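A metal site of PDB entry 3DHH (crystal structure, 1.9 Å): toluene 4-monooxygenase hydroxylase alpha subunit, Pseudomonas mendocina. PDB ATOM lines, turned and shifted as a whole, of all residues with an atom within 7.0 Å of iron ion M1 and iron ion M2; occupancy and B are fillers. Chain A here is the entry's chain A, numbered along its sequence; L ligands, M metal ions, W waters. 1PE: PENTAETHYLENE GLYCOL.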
ATOM      1  N   ILE A 100     -24.578  -7.768 -29.275  1.00  0.00           N
ATOM      2  CA  ILE A 100     -23.673  -6.703 -28.790  1.00  0.00           C
ATOM      3  C   ILE A 100     -23.516  -5.458 -29.653  1.00  0.00           C
ATOM      4  O   ILE A 100     -23.555  -4.356 -29.115  1.00  0.00           O
ATOM      5  CB  ILE A 100     -22.262  -7.287 -28.444  1.00  0.00           C
ATOM      6  CG1 ILE A 100     -22.357  -8.201 -27.225  1.00  0.00           C
ATOM      7  CG2 ILE A 100     -21.204  -6.192 -28.246  1.00  0.00           C
ATOM      8  CD1 ILE A 100     -23.038  -7.607 -25.987  1.00  0.00           C
ATOM      9  N   GLY A 103     -26.045  -2.649 -29.464  1.00  0.00           N
ATOM     10  CA  GLY A 103     -26.082  -2.261 -28.032  1.00  0.00           C
ATOM     11  C   GLY A 103     -24.916  -1.352 -27.619  1.00  0.00           C
ATOM     12  O   GLY A 103     -25.133  -0.390 -26.904  1.00  0.00           O
ATOM     13  N   GLU A 104     -23.699  -1.656 -28.089  1.00  0.00           N
ATOM     14  CA  GLU A 104     -22.556  -0.739 -27.948  1.00  0.00           C
ATOM     15  C   GLU A 104     -22.919   0.630 -28.487  1.00  0.00           C
ATOM     16  O   GLU A 104     -22.726   1.644 -27.831  1.00  0.00           O
ATOM     17  CB  GLU A 104     -21.357  -1.279 -28.764  1.00  0.00           C
ATOM     18  CG  GLU A 104     -20.862  -2.619 -28.237  1.00  0.00           C
ATOM     19  CD  GLU A 104     -19.801  -2.492 -27.165  1.00  0.00           C
ATOM     20  OE1 GLU A 104     -19.074  -3.470 -26.911  1.00  0.00           O
ATOM     21  OE2 GLU A 104     -19.702  -1.432 -26.554  1.00  0.00           O
ATOM     22  N   TYR A 105     -23.458   0.687 -29.702  1.00  0.00           N
ATOM     23  CA  TYR A 105     -23.867   1.971 -30.242  1.00  0.00           C
ATOM     24  C   TYR A 105     -24.972   2.689 -29.402  1.00  0.00           C
ATOM     25  O   TYR A 105     -24.908   3.899 -29.211  1.00  0.00           O
ATOM     26  CB  TYR A 105     -24.273   1.828 -31.731  1.00  0.00           C
ATOM     27  CG  TYR A 105     -24.468   3.177 -32.360  1.00  0.00           C
ATOM     28  CD1 TYR A 105     -23.375   3.941 -32.739  1.00  0.00           C
ATOM     29  CD2 TYR A 105     -25.741   3.722 -32.481  1.00  0.00           C
ATOM     30  CE1 TYR A 105     -23.550   5.217 -33.288  1.00  0.00           C
ATOM     31  CE2 TYR A 105     -25.934   5.001 -33.038  1.00  0.00           C
ATOM     32  CZ  TYR A 105     -24.826   5.742 -33.408  1.00  0.00           C
ATOM     33  OH  TYR A 105     -24.970   7.003 -33.932  1.00  0.00           O
ATOM     34  N   ALA A 107     -25.098   2.426 -26.216  1.00  0.00           N
ATOM     35  CA  ALA A 107     -24.329   2.948 -25.064  1.00  0.00           C
ATOM     36  C   ALA A 107     -23.729   4.355 -25.296  1.00  0.00           C
ATOM     37  O   ALA A 107     -23.467   5.080 -24.323  1.00  0.00           O
ATOM     38  CB  ALA A 107     -23.260   1.947 -24.618  1.00  0.00           C
ATOM     39  N   GLU A 111     -23.760   7.487 -22.407  1.00  0.00           N
ATOM     40  CA  GLU A 111     -22.613   8.365 -22.163  1.00  0.00           C
ATOM     41  C   GLU A 111     -22.960   9.805 -22.538  1.00  0.00           C
ATOM     42  O   GLU A 111     -22.620  10.746 -21.791  1.00  0.00           O
ATOM     43  CB  GLU A 111     -21.383   7.882 -22.927  1.00  0.00           C
ATOM     44  CG  GLU A 111     -20.820   6.509 -22.445  1.00  0.00           C
ATOM     45  CD  GLU A 111     -20.001   6.621 -21.126  1.00  0.00           C
ATOM     46  OE1 GLU A 111     -19.638   7.734 -20.723  1.00  0.00           O
ATOM     47  OE2 GLU A 111     -19.705   5.579 -20.493  1.00  0.00           O
ATOM     48  N   GLY A 130     -16.154   8.556 -23.133  1.00  0.00           N
ATOM     49  CA  GLY A 130     -17.002   7.349 -23.145  1.00  0.00           C
ATOM     50  C   GLY A 130     -17.892   7.271 -24.366  1.00  0.00           C
ATOM     51  O   GLY A 130     -18.097   6.180 -24.922  1.00  0.00           O
ATOM     52  N   ASP A 133     -15.563   6.080 -27.085  1.00  0.00           N
ATOM     53  CA  ASP A 133     -15.256   4.674 -26.883  1.00  0.00           C
ATOM     54  C   ASP A 133     -16.417   3.753 -27.413  1.00  0.00           C
ATOM     55  O   ASP A 133     -16.194   2.791 -28.017  1.00  0.00           O
ATOM     56  CB  ASP A 133     -15.072   4.367 -25.404  1.00  0.00           C
ATOM     57  CG  ASP A 133     -13.831   4.983 -24.791  1.00  0.00           C
ATOM     58  OD1 ASP A 133     -12.916   5.375 -25.451  1.00  0.00           O
ATOM     59  OD2 ASP A 133     -13.799   5.021 -23.592  1.00  0.00           O
ATOM     60  N   GLU A 134     -17.649   4.116 -27.140  1.00  0.00           N
ATOM     61  CA  GLU A 134     -18.742   3.247 -27.504  1.00  0.00           C
ATOM     62  C   GLU A 134     -18.991   3.331 -28.992  1.00  0.00           C
ATOM     63  O   GLU A 134     -19.294   2.397 -29.570  1.00  0.00           O
ATOM     64  CB  GLU A 134     -20.013   3.464 -26.690  1.00  0.00           C
ATOM     65  CG  GLU A 134     -19.861   3.447 -25.207  1.00  0.00           C
ATOM     66  CD  GLU A 134     -19.487   2.108 -24.633  1.00  0.00           C
ATOM     67  OE1 GLU A 134     -19.119   1.241 -25.358  1.00  0.00           O
ATOM     68  OE2 GLU A 134     -19.612   1.927 -23.482  1.00  0.00           O
ATOM     69  N   LEU A 135     -18.783   4.492 -29.575  1.00  0.00           N
ATOM     70  CA  LEU A 135     -18.748   4.610 -31.020  1.00  0.00           C
ATOM     71  C   LEU A 135     -17.725   3.617 -31.598  1.00  0.00           C
ATOM     72  O   LEU A 135     -18.027   2.921 -32.470  1.00  0.00           O
ATOM     73  CB  LEU A 135     -18.415   6.007 -31.451  1.00  0.00           C
ATOM     74  CG  LEU A 135     -18.493   6.275 -32.936  1.00  0.00           C
ATOM     75  CD1 LEU A 135     -19.840   6.064 -33.489  1.00  0.00           C
ATOM     76  CD2 LEU A 135     -17.996   7.585 -33.268  1.00  0.00           C
ATOM     77  N   HIS A 137     -16.610   0.880 -30.300  1.00  0.00           N
ATOM     78  CA  HIS A 137     -17.011  -0.519 -30.094  1.00  0.00           C
ATOM     79  C   HIS A 137     -18.145  -0.936 -31.028  1.00  0.00           C
ATOM     80  O   HIS A 137     -18.148  -2.050 -31.551  1.00  0.00           O
ATOM     81  CB  HIS A 137     -17.461  -0.721 -28.664  1.00  0.00           C
ATOM     82  CG  HIS A 137     -16.390  -0.384 -27.662  1.00  0.00           C
ATOM     83  ND1 HIS A 137     -16.636  -0.266 -26.305  1.00  0.00           N
ATOM     84  CD2 HIS A 137     -15.079  -0.119 -27.838  1.00  0.00           C
ATOM     85  CE1 HIS A 137     -15.508   0.054 -25.692  1.00  0.00           C
ATOM     86  NE2 HIS A 137     -14.550   0.161 -26.603  1.00  0.00           N
ATOM     87  N   GLY A 138     -19.097  -0.020 -31.220  1.00  0.00           N
ATOM     88  CA  GLY A 138     -20.173  -0.265 -32.200  1.00  0.00           C
ATOM     89  C   GLY A 138     -19.613  -0.445 -33.592  1.00  0.00           C
ATOM     90  O   GLY A 138     -20.018  -1.375 -34.313  1.00  0.00           O
ATOM     91  N   GLN A 141     -17.542  -3.770 -34.006  1.00  0.00           N
ATOM     92  CA  GLN A 141     -18.320  -5.018 -33.940  1.00  0.00           C
ATOM     93  C   GLN A 141     -19.377  -5.106 -35.035  1.00  0.00           C
ATOM     94  O   GLN A 141     -20.100  -6.092 -35.101  1.00  0.00           O
ATOM     95  CB  GLN A 141     -18.903  -5.209 -32.557  1.00  0.00           C
ATOM     96  CG  GLN A 141     -17.765  -5.573 -31.584  1.00  0.00           C
ATOM     97  CD  GLN A 141     -18.127  -5.474 -30.122  1.00  0.00           C
ATOM     98  OE1 GLN A 141     -18.516  -4.396 -29.599  1.00  0.00           O
ATOM     99  NE2 GLN A 141     -17.960  -6.574 -29.440  1.00  0.00           N
ATOM    100  N   LEU A 192     -25.142   1.646 -15.383  1.00  0.00           N
ATOM    101  CA  LEU A 192     -24.275   1.287 -16.509  1.00  0.00           C
ATOM    102  C   LEU A 192     -22.789   1.270 -16.105  1.00  0.00           C
ATOM    103  O   LEU A 192     -22.169   0.213 -16.139  1.00  0.00           O
ATOM    104  CB  LEU A 192     -24.476   2.190 -17.711  1.00  0.00           C
ATOM    105  CG  LEU A 192     -23.502   1.965 -18.880  1.00  0.00           C
ATOM    106  CD1 LEU A 192     -23.623   0.514 -19.455  1.00  0.00           C
ATOM    107  CD2 LEU A 192     -23.793   3.027 -19.971  1.00  0.00           C
ATOM    108  N   THR A 193     -22.203   2.405 -15.773  1.00  0.00           N
ATOM    109  CA  THR A 193     -20.723   2.424 -15.692  1.00  0.00           C
ATOM    110  C   THR A 193     -20.216   1.642 -14.490  1.00  0.00           C
ATOM    111  O   THR A 193     -19.242   0.909 -14.611  1.00  0.00           O
ATOM    112  CB  THR A 193     -20.100   3.829 -15.750  1.00  0.00           C
ATOM    113  OG1 THR A 193     -20.428   4.566 -14.560  1.00  0.00           O
ATOM    114  CG2 THR A 193     -20.649   4.578 -16.944  1.00  0.00           C
ATOM    115  N   PHE A 196     -22.878  -2.537 -14.460  1.00  0.00           N
ATOM    116  CA  PHE A 196     -22.695  -3.351 -15.650  1.00  0.00           C
ATOM    117  C   PHE A 196     -21.239  -3.390 -16.140  1.00  0.00           C
ATOM    118  O   PHE A 196     -20.713  -4.497 -16.406  1.00  0.00           O
ATOM    119  CB  PHE A 196     -23.658  -2.856 -16.746  1.00  0.00           C
ATOM    120  CG  PHE A 196     -23.760  -3.774 -17.928  1.00  0.00           C
ATOM    121  CD1 PHE A 196     -24.325  -5.037 -17.825  1.00  0.00           C
ATOM    122  CD2 PHE A 196     -23.313  -3.355 -19.171  1.00  0.00           C
ATOM    123  CE1 PHE A 196     -24.406  -5.856 -18.942  1.00  0.00           C
ATOM    124  CE2 PHE A 196     -23.415  -4.161 -20.287  1.00  0.00           C
ATOM    125  CZ  PHE A 196     -23.966  -5.395 -20.181  1.00  0.00           C
ATOM    126  N   GLU A 197     -20.597  -2.232 -16.255  1.00  0.00           N
ATOM    127  CA  GLU A 197     -19.301  -2.137 -16.934  1.00  0.00           C
ATOM    128  C   GLU A 197     -18.104  -2.492 -16.045  1.00  0.00           C
ATOM    129  O   GLU A 197     -17.054  -2.830 -16.572  1.00  0.00           O
ATOM    130  CB  GLU A 197     -19.093  -0.753 -17.537  1.00  0.00           C
ATOM    131  CG  GLU A 197     -20.099  -0.404 -18.639  1.00  0.00           C
ATOM    132  CD  GLU A 197     -19.838   1.001 -19.254  1.00  0.00           C
ATOM    133  OE1 GLU A 197     -19.590   1.958 -18.494  1.00  0.00           O
ATOM    134  OE2 GLU A 197     -19.871   1.156 -20.481  1.00  0.00           O
ATOM    135  N   THR A 201     -19.426  -7.019 -17.736  1.00  0.00           N
ATOM    136  CA  THR A 201     -18.910  -7.081 -19.136  1.00  0.00           C
ATOM    137  C   THR A 201     -17.591  -7.830 -19.217  1.00  0.00           C
ATOM    138  O   THR A 201     -17.295  -8.427 -20.259  1.00  0.00           O
ATOM    139  CB  THR A 201     -18.754  -5.721 -19.803  1.00  0.00           C
ATOM    140  OG1 THR A 201     -17.886  -4.918 -19.027  1.00  0.00           O
ATOM    141  CG2 THR A 201     -20.112  -5.020 -19.952  1.00  0.00           C
ATOM    142  N   PHE A 205     -16.197 -10.041 -22.438  1.00  0.00           N
ATOM    143  CA  PHE A 205     -15.120  -9.464 -23.177  1.00  0.00           C
ATOM    144  C   PHE A 205     -13.713  -9.944 -22.733  1.00  0.00           C
ATOM    145  O   PHE A 205     -12.729  -9.726 -23.414  1.00  0.00           O
ATOM    146  CB  PHE A 205     -15.206  -7.968 -23.119  1.00  0.00           C
ATOM    147  CG  PHE A 205     -16.298  -7.386 -23.941  1.00  0.00           C
ATOM    148  CD1 PHE A 205     -17.543  -7.209 -23.428  1.00  0.00           C
ATOM    149  CD2 PHE A 205     -16.091  -6.999 -25.228  1.00  0.00           C
ATOM    150  CE1 PHE A 205     -18.546  -6.711 -24.182  1.00  0.00           C
ATOM    151  CE2 PHE A 205     -17.103  -6.509 -25.964  1.00  0.00           C
ATOM    152  CZ  PHE A 205     -18.320  -6.336 -25.417  1.00  0.00           C
ATOM    153  N   ILE A 227     -11.190  -3.852 -26.810  1.00  0.00           N
ATOM    154  CA  ILE A 227     -12.436  -3.180 -26.418  1.00  0.00           C
ATOM    155  C   ILE A 227     -12.546  -3.021 -24.877  1.00  0.00           C
ATOM    156  O   ILE A 227     -12.877  -1.942 -24.362  1.00  0.00           O
ATOM    157  CB  ILE A 227     -13.664  -3.949 -26.990  1.00  0.00           C
ATOM    158  CG1 ILE A 227     -13.785  -3.684 -28.505  1.00  0.00           C
ATOM    159  CG2 ILE A 227     -14.964  -3.495 -26.253  1.00  0.00           C
ATOM    160  CD1 ILE A 227     -14.904  -4.577 -29.270  1.00  0.00           C
ATOM    161  N   GLN A 228     -12.249  -4.091 -24.131  1.00  0.00           N
ATOM    162  CA  GLN A 228     -12.356  -3.994 -22.670  1.00  0.00           C
ATOM    163  C   GLN A 228     -11.330  -2.987 -22.053  1.00  0.00           C
ATOM    164  O   GLN A 228     -11.561  -2.482 -20.942  1.00  0.00           O
ATOM    165  CB  GLN A 228     -12.258  -5.387 -22.013  1.00  0.00           C
ATOM    166  CG  GLN A 228     -12.941  -5.449 -20.629  1.00  0.00           C
ATOM    167  CD  GLN A 228     -14.464  -5.247 -20.683  1.00  0.00           C
ATOM    168  OE1 GLN A 228     -15.011  -4.942 -21.739  1.00  0.00           O
ATOM    169  NE2 GLN A 228     -15.132  -5.408 -19.546  1.00  0.00           N
ATOM    170  N   ASP A 230     -10.906  -0.006 -23.100  1.00  0.00           N
ATOM    171  CA  ASP A 230     -11.690   1.231 -23.054  1.00  0.00           C
ATOM    172  C   ASP A 230     -12.668   1.244 -21.900  1.00  0.00           C
ATOM    173  O   ASP A 230     -12.778   2.219 -21.173  1.00  0.00           O
ATOM    174  CB  ASP A 230     -12.485   1.441 -24.359  1.00  0.00           C
ATOM    175  CG  ASP A 230     -11.611   1.616 -25.584  1.00  0.00           C
ATOM    176  OD1 ASP A 230     -10.518   2.217 -25.468  1.00  0.00           O
ATOM    177  OD2 ASP A 230     -12.026   1.117 -26.653  1.00  0.00           O
ATOM    178  N   GLU A 231     -13.378   0.129 -21.742  1.00  0.00           N
ATOM    179  CA  GLU A 231     -14.356  -0.073 -20.667  1.00  0.00           C
ATOM    180  C   GLU A 231     -13.705   0.169 -19.322  1.00  0.00           C
ATOM    181  O   GLU A 231     -14.269   0.857 -18.468  1.00  0.00           O
ATOM    182  CB  GLU A 231     -14.885  -1.517 -20.740  1.00  0.00           C
ATOM    183  CG  GLU A 231     -15.957  -1.856 -19.726  1.00  0.00           C
ATOM    184  CD  GLU A 231     -17.352  -1.573 -20.267  1.00  0.00           C
ATOM    185  OE1 GLU A 231     -18.197  -2.487 -20.282  1.00  0.00           O
ATOM    186  OE2 GLU A 231     -17.607  -0.454 -20.716  1.00  0.00           O
ATOM    187  N   SER A 232     -12.511  -0.382 -19.126  1.00  0.00           N
ATOM    188  CA  SER A 232     -11.780  -0.176 -17.875  1.00  0.00           C
ATOM    189  C   SER A 232     -11.571   1.287 -17.470  1.00  0.00           C
ATOM    190  O   SER A 232     -11.623   1.583 -16.265  1.00  0.00           O
ATOM    191  CB  SER A 232     -10.473  -0.942 -17.861  1.00  0.00           C
ATOM    192  OG  SER A 232     -10.824  -2.325 -17.962  1.00  0.00           O
ATOM    193  N   HIS A 234     -13.661   4.082 -18.991  1.00  0.00           N
ATOM    194  CA  HIS A 234     -14.890   4.857 -18.852  1.00  0.00           C
ATOM    195  C   HIS A 234     -15.775   4.265 -17.779  1.00  0.00           C
ATOM    196  O   HIS A 234     -16.614   4.983 -17.241  1.00  0.00           O
ATOM    197  CB  HIS A 234     -15.657   5.123 -20.150  1.00  0.00           C
ATOM    198  CG  HIS A 234     -16.174   3.898 -20.848  1.00  0.00           C
ATOM    199  ND1 HIS A 234     -15.751   3.560 -22.110  1.00  0.00           N
ATOM    200  CD2 HIS A 234     -17.132   2.979 -20.507  1.00  0.00           C
ATOM    201  CE1 HIS A 234     -16.406   2.475 -22.519  1.00  0.00           C
ATOM    202  NE2 HIS A 234     -17.237   2.105 -21.563  1.00  0.00           N
ATOM    203  N   ALA A 235     -15.567   2.980 -17.433  1.00  0.00           N
ATOM    204  CA  ALA A 235     -16.374   2.385 -16.338  1.00  0.00           C
ATOM    205  C   ALA A 235     -16.087   3.052 -14.990  1.00  0.00           C
ATOM    206  O   ALA A 235     -16.907   2.983 -14.078  1.00  0.00           O
ATOM    207  CB  ALA A 235     -16.228   0.902 -16.252  1.00  0.00           C
HETATM  208  OH4 1PE L   1     -20.279  -1.134 -23.926  1.00  0.00           O
HETATM  209  C14 1PE L   1     -22.369  -1.494 -22.862  1.00  0.00           C
HETATM  210  C24 1PE L   1     -20.888  -1.210 -22.640  1.00  0.00           C
HETATM  211  OH5 1PE L   1     -22.631  -2.154 -24.113  1.00  0.00           O
HETATM  212  C15 1PE L   1     -23.114  -4.443 -24.494  1.00  0.00           C
HETATM  213  C25 1PE L   1     -22.009  -3.448 -24.289  1.00  0.00           C
HETATM  214  OH6 1PE L   1     -24.218  -3.774 -25.132  1.00  0.00           O
HETATM  215  C26 1PE L   1     -24.805  -4.627 -26.089  1.00  0.00           C
HETATM  216 FE    FE M   1     -18.469  -0.748 -25.067  1.00  0.00          FE
HETATM  217 FE    FE M   2     -18.624   0.522 -22.042  1.00  0.00          FE
HETATM  218  O   HOH W   1     -17.821  -2.889 -24.828  1.00  0.00           O
HETATM  219  O   HOH W   2     -17.447  -0.376 -23.239  1.00  0.00           O
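Of the 26 residues printed, 4 come within 4 Å of iron ion M2. The nearest printed residue that does not touch iron ion M2 is His 137 (4.8 Å).
A ring nitrogen (ND1) of His 234 sits at hydrogen-bond distance from the side-chain carboxylate (OD2) of Asp 133 (2.9 Å). A ring nitrogen (ND1) of His 234 is in hydrogen-bond range of the backbone carbonyl oxygen (O) of Asp 230, at 3.4 Å. The backbone carbonyl oxygen (O) of Asp 133 lies close to a ring nitrogen (NE2) of His 137 (3.4 Å). The side-chain hydroxyl (OG1) of Thr 201 sits at hydrogen-bond distance from the backbone carbonyl oxygen (O) of Glu 197, at 3.3 Å. OE1 of Gln 141 sits close to OE1 of Glu 104 (2.9 Å). The backbone NH (N) of Glu 197 sits at hydrogen-bond distance from the backbone carbonyl oxygen (O) of Leu 192, at 2.9 Å. OE1 of Glu 231 sits at hydrogen-bond distance from OG1 of Thr 201, 2.8 Å away. A ring nitrogen (NE2) of His 137 lies within hydrogen-bond range of the backbone carbonyl oxygen of Ile 227 (3.5 Å).
Iron ion M1 is bound by OE2 of Glu 104 (2.0 Å), OE1 of Glu 134 (2.1 Å), water W2 (2.1 Å), OH4 of the ligand (2.2 Å), water W1 (2.2 Å) and ND1 of His 137 (2.3 Å). Iron ion M1 has six donor atoms within binding distance.
Of the 26 residues printed, 3 come within 4 Å of iron ion M1.
Water W2 is bound to iron ion M2. The side-chain carboxylate (OE2) of Glu 231 is bound to iron ion M2 (1.9 Å). Iron ion M2 is bound by the side-chain carboxylate (OE2) of Glu 197, at 2.1 Å. Iron ion M2 is bound by NE2 of His 234, at 2.2 Å. The side-chain carboxylate (OE2) of Glu 134 is bound to iron ion M2 (2.2 Å).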
